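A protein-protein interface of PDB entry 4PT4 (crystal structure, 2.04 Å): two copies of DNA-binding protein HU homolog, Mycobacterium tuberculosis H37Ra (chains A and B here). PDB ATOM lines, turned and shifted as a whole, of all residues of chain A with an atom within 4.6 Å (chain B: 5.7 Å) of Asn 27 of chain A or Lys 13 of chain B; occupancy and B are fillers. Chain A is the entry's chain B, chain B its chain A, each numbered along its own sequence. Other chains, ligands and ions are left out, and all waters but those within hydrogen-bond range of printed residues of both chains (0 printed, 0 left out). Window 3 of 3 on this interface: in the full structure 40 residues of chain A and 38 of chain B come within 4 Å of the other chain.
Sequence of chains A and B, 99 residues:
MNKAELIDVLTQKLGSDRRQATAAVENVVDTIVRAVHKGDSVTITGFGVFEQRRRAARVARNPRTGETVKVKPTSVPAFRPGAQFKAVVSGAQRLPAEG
NZ of Lys 13 of chain B lies within salt-bridge range of OD2 of Asp 30 of chain A (2.9 Å). The side-chain hydroxyl (OG1) of Thr 31 of chain A lies within hydrogen-bond range of the side-chain amino group (NZ) of Lys 13 of chain B (3.0 Å).
The backbone carbonyl oxygen (O) of Ala 23 of chain A is in hydrogen-bond range of the side-chain amide nitrogen (ND2) of Asn 27 of chain A (3.0 Å). The side-chain hydroxyl (OG1) of Thr 31 of chain A sits at hydrogen-bond distance from the backbone carbonyl oxygen (O) of Asn 27 of chain A (2.7 Å).
Leu 14 of chain B touches Ala 23 of chain A. Leu 14 of chain B touches Ala 24 of chain A. Asn 27 of chain A touches Leu 10 of chain B (CB to CD1, 3.8 Å). OD1 of Asn 27 of chain A touches CD of Lys 13 of chain B (3.4 Å). CD2 of Leu 10 of chain B touches CG2 of Val 28 of chain A, 3.8 Å away. Leu 6 of chain B touches Thr 31 of chain A. CG1 of Val 9 of chain B touches OG1 of Thr 31 of chain A, 3.5 Å away.
Of the printed residues of chain B, Asn 27 of chain A touches Leu 10 and Lys 13. Of the printed residues of chain B, Asp 30 of chain A touches Lys 13. Printed residues of chain A within 4 Å of Leu 6 of chain B: Thr 31. The nearest printed residue of chain A that does not touch Lys 13 of chain B is Val 28 of chain A (6.2 Å). The nearest printed residue of chain B that does not touch Ala 23 of chain A is Leu 10 of chain B (5.0 Å).
Of the 9 printed residues of chain B, 5 touch a printed residue of chain A. Among the printed residues, 9 pairs touch across the chains. Among the printed residues, Asp or Glu carboxylates within 4 Å of a Lys or Arg side-chain nitrogen of the other chain: Asp 30 of chain A with Lys 13 of chain B.
No position is printed for both chains. Of the 9 pairs that touch across the chains among the printed residues, none has its exchanged pair printed and touching as well.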
ATOM      1  N   ALA A  23     -14.051   6.994 -12.229  1.00  0.00           N
ATOM      2  CA  ALA A  23     -13.368   7.618 -11.121  1.00  0.00           C
ATOM      3  C   ALA A  23     -12.306   6.675 -10.589  1.00  0.00           C
ATOM      4  O   ALA A  23     -11.204   7.097 -10.247  1.00  0.00           O
ATOM      5  CB  ALA A  23     -14.354   7.984 -10.015  1.00  0.00           C
ATOM      6  N   ALA A  24     -12.647   5.395 -10.508  1.00  0.00           N
ATOM      7  CA  ALA A  24     -11.715   4.389 -10.018  1.00  0.00           C
ATOM      8  C   ALA A  24     -10.449   4.352 -10.831  1.00  0.00           C
ATOM      9  O   ALA A  24      -9.365   4.412 -10.276  1.00  0.00           O
ATOM     10  CB  ALA A  24     -12.362   3.023 -10.045  1.00  0.00           C
ATOM     11  N   VAL A  25     -10.595   4.260 -12.159  1.00  0.00           N
ATOM     12  CA  VAL A  25      -9.446   4.176 -13.030  1.00  0.00           C
ATOM     13  C   VAL A  25      -8.624   5.470 -12.928  1.00  0.00           C
ATOM     14  O   VAL A  25      -7.404   5.454 -12.751  1.00  0.00           O
ATOM     15  CB  VAL A  25      -9.867   3.856 -14.474  1.00  0.00           C
ATOM     16  CG1 VAL A  25      -8.679   3.960 -15.445  1.00  0.00           C
ATOM     17  CG2 VAL A  25     -10.463   2.462 -14.548  1.00  0.00           C
ATOM     18  N   GLU A  26      -9.287   6.598 -12.991  1.00  0.00           N
ATOM     19  CA  GLU A  26      -8.552   7.853 -13.039  1.00  0.00           C
ATOM     20  C   GLU A  26      -7.855   8.174 -11.733  1.00  0.00           C
ATOM     21  O   GLU A  26      -6.781   8.801 -11.710  1.00  0.00           O
ATOM     22  CB  GLU A  26      -9.479   8.962 -13.480  1.00  0.00           C
ATOM     23  CG  GLU A  26      -9.930   8.754 -14.930  1.00  0.00           C
ATOM     24  CD  GLU A  26     -10.660   9.944 -15.487  1.00  0.00           C
ATOM     25  OE1 GLU A  26     -10.970  10.850 -14.691  1.00  0.00           O
ATOM     26  OE2 GLU A  26     -10.925   9.991 -16.708  1.00  0.00           O
ATOM     27  N   ASN A  27      -8.429   7.707 -10.635  1.00  0.00           N
ATOM     28  CA  ASN A  27      -7.855   7.994  -9.326  1.00  0.00           C
ATOM     29  C   ASN A  27      -6.854   6.943  -8.892  1.00  0.00           C
ATOM     30  O   ASN A  27      -5.947   7.237  -8.087  1.00  0.00           O
ATOM     31  CB  ASN A  27      -8.964   8.240  -8.313  1.00  0.00           C
ATOM     32  CG  ASN A  27      -9.522   9.649  -8.439  1.00  0.00           C
ATOM     33  OD1 ASN A  27      -8.872  10.628  -8.048  1.00  0.00           O
ATOM     34  ND2 ASN A  27     -10.685   9.760  -9.044  1.00  0.00           N
ATOM     35  N   VAL A  28      -6.971   5.733  -9.446  1.00  0.00           N
ATOM     36  CA  VAL A  28      -5.881   4.824  -9.292  1.00  0.00           C
ATOM     37  C   VAL A  28      -4.674   5.433  -9.992  1.00  0.00           C
ATOM     38  O   VAL A  28      -3.588   5.451  -9.454  1.00  0.00           O
ATOM     39  CB  VAL A  28      -6.110   3.431  -9.906  1.00  0.00           C
ATOM     40  CG1 VAL A  28      -4.759   2.732  -9.988  1.00  0.00           C
ATOM     41  CG2 VAL A  28      -7.066   2.636  -9.059  1.00  0.00           C
ATOM     42  N   VAL A  29      -4.877   5.873 -11.220  1.00  0.00           N
ATOM     43  CA  VAL A  29      -3.814   6.476 -12.015  1.00  0.00           C
ATOM     44  C   VAL A  29      -3.151   7.658 -11.270  1.00  0.00           C
ATOM     45  O   VAL A  29      -1.901   7.733 -11.116  1.00  0.00           O
ATOM     46  CB  VAL A  29      -4.375   6.907 -13.412  1.00  0.00           C
ATOM     47  CG1 VAL A  29      -3.460   7.888 -14.113  1.00  0.00           C
ATOM     48  CG2 VAL A  29      -4.569   5.690 -14.303  1.00  0.00           C
ATOM     49  N   ASP A  30      -3.992   8.570 -10.803  1.00  0.00           N
ATOM     50  CA  ASP A  30      -3.515   9.802 -10.163  1.00  0.00           C
ATOM     51  C   ASP A  30      -2.729   9.474  -8.885  1.00  0.00           C
ATOM     52  O   ASP A  30      -1.778  10.188  -8.537  1.00  0.00           O
ATOM     53  CB  ASP A  30      -4.721  10.669  -9.840  1.00  0.00           C
ATOM     54  CG  ASP A  30      -4.364  11.948  -9.076  1.00  0.00           C
ATOM     55  OD1 ASP A  30      -3.908  12.914  -9.717  1.00  0.00           O
ATOM     56  OD2 ASP A  30      -4.595  12.011  -7.832  1.00  0.00           O
ATOM     57  N   THR A  31      -3.150   8.432  -8.161  1.00  0.00           N
ATOM     58  CA  THR A  31      -2.493   8.081  -6.907  1.00  0.00           C
ATOM     59  C   THR A  31      -1.076   7.559  -7.218  1.00  0.00           C
ATOM     60  O   THR A  31      -0.105   7.983  -6.608  1.00  0.00           O
ATOM     61  CB  THR A  31      -3.279   7.054  -6.079  1.00  0.00           C
ATOM     62  OG1 THR A  31      -4.587   7.556  -5.757  1.00  0.00           O
ATOM     63  CG2 THR A  31      -2.551   6.767  -4.773  1.00  0.00           C
ATOM     64  N   LEU B   6      -2.343   2.390  -1.001  1.00  0.00           N
ATOM     65  CA  LEU B   6      -2.941   2.787  -2.274  1.00  0.00           C
ATOM     66  C   LEU B   6      -4.454   2.710  -2.107  1.00  0.00           C
ATOM     67  O   LEU B   6      -5.170   3.609  -2.513  1.00  0.00           O
ATOM     68  CB  LEU B   6      -2.425   1.893  -3.439  1.00  0.00           C
ATOM     69  CG  LEU B   6      -3.204   1.850  -4.758  1.00  0.00           C
ATOM     70  CD1 LEU B   6      -3.245   3.245  -5.363  1.00  0.00           C
ATOM     71  CD2 LEU B   6      -2.580   0.859  -5.743  1.00  0.00           C
ATOM     72  N   ASP B   8      -6.140   2.772   0.789  1.00  0.00           N
ATOM     73  CA  ASP B   8      -6.614   3.777   1.737  1.00  0.00           C
ATOM     74  C   ASP B   8      -6.794   5.092   1.023  1.00  0.00           C
ATOM     75  O   ASP B   8      -7.838   5.731   1.167  1.00  0.00           O
ATOM     76  CB  ASP B   8      -5.674   3.936   2.915  1.00  0.00           C
ATOM     77  CG  ASP B   8      -5.563   2.680   3.755  1.00  0.00           C
ATOM     78  OD1 ASP B   8      -6.486   1.816   3.741  1.00  0.00           O
ATOM     79  OD2 ASP B   8      -4.513   2.556   4.423  1.00  0.00           O
ATOM     80  N   VAL B   9      -5.811   5.462   0.205  1.00  0.00           N
ATOM     81  CA  VAL B   9      -5.885   6.702  -0.603  1.00  0.00           C
ATOM     82  C   VAL B   9      -7.102   6.703  -1.538  1.00  0.00           C
ATOM     83  O   VAL B   9      -7.918   7.654  -1.569  1.00  0.00           O
ATOM     84  CB  VAL B   9      -4.593   6.961  -1.403  1.00  0.00           C
ATOM     85  CG1 VAL B   9      -4.752   8.175  -2.322  1.00  0.00           C
ATOM     86  CG2 VAL B   9      -3.390   7.177  -0.474  1.00  0.00           C
ATOM     87  N   LEU B  10      -7.265   5.608  -2.257  1.00  0.00           N
ATOM     88  CA  LEU B  10      -8.344   5.502  -3.219  1.00  0.00           C
ATOM     89  C   LEU B  10      -9.724   5.564  -2.549  1.00  0.00           C
ATOM     90  O   LEU B  10     -10.674   6.177  -3.074  1.00  0.00           O
ATOM     91  CB  LEU B  10      -8.172   4.213  -4.027  1.00  0.00           C
ATOM     92  CG  LEU B  10      -9.156   4.031  -5.178  1.00  0.00           C
ATOM     93  CD1 LEU B  10      -9.033   5.114  -6.238  1.00  0.00           C
ATOM     94  CD2 LEU B  10      -8.973   2.645  -5.797  1.00  0.00           C
ATOM     95  N   THR B  11      -9.839   4.932  -1.387  1.00  0.00           N
ATOM     96  CA  THR B  11     -11.044   5.018  -0.579  1.00  0.00           C
ATOM     97  C   THR B  11     -11.451   6.498  -0.374  1.00  0.00           C
ATOM     98  O   THR B  11     -12.578   6.886  -0.687  1.00  0.00           O
ATOM     99  CB  THR B  11     -10.867   4.251   0.767  1.00  0.00           C
ATOM    100  OG1 THR B  11     -10.722   2.856   0.493  1.00  0.00           O
ATOM    101  CG2 THR B  11     -12.070   4.360   1.623  1.00  0.00           C
ATOM    102  N   GLN B  12     -10.533   7.346   0.071  1.00  0.00           N
ATOM    103  CA  GLN B  12     -10.909   8.751   0.341  1.00  0.00           C
ATOM    104  C   GLN B  12     -11.263   9.486  -0.967  1.00  0.00           C
ATOM    105  O   GLN B  12     -12.168  10.316  -0.998  1.00  0.00           O
ATOM    106  CB  GLN B  12      -9.796   9.474   1.081  1.00  0.00           C
ATOM    107  CG  GLN B  12      -9.318   8.772   2.363  1.00  0.00           C
ATOM    108  CD  GLN B  12     -10.366   8.670   3.508  1.00  0.00           C
ATOM    109  OE1 GLN B  12     -10.994   9.663   3.918  1.00  0.00           O
ATOM    110  NE2 GLN B  12     -10.515   7.468   4.048  1.00  0.00           N
ATOM    111  N   LYS B  13     -10.591   9.161  -2.067  1.00  0.00           N
ATOM    112  CA  LYS B  13     -10.895   9.840  -3.312  1.00  0.00           C
ATOM    113  C   LYS B  13     -12.245   9.453  -3.854  1.00  0.00           C
ATOM    114  O   LYS B  13     -12.980  10.295  -4.335  1.00  0.00           O
ATOM    115  CB  LYS B  13      -9.801   9.591  -4.346  1.00  0.00           C
ATOM    116  CG  LYS B  13      -8.483  10.263  -3.973  1.00  0.00           C
ATOM    117  CD  LYS B  13      -7.396  10.125  -5.024  1.00  0.00           C
ATOM    118  CE  LYS B  13      -6.169  10.900  -4.562  1.00  0.00           C
ATOM    119  NZ  LYS B  13      -4.926  10.533  -5.303  1.00  0.00           N
ATOM    120  N   LEU B  14     -12.549   8.159  -3.805  1.00  0.00           N
ATOM    121  CA  LEU B  14     -13.798   7.667  -4.323  1.00  0.00           C
ATOM    122  C   LEU B  14     -14.957   7.880  -3.381  1.00  0.00           C
ATOM    123  O   LEU B  14     -16.081   7.808  -3.816  1.00  0.00           O
ATOM    124  CB  LEU B  14     -13.708   6.173  -4.592  1.00  0.00           C
ATOM    125  CG  LEU B  14     -12.793   5.756  -5.720  1.00  0.00           C
ATOM    126  CD1 LEU B  14     -13.099   4.293  -5.999  1.00  0.00           C
ATOM    127  CD2 LEU B  14     -12.938   6.615  -6.967  1.00  0.00           C
ATOM    128  N   GLY B  15     -14.678   8.065  -2.090  1.00  0.00           N
ATOM    129  CA  GLY B  15     -15.717   8.138  -1.067  1.00  0.00           C
ATOM    130  C   GLY B  15     -16.468   6.836  -0.964  1.00  0.00           C
ATOM    131  O   GLY B  15     -17.693   6.814  -0.785  1.00  0.00           O
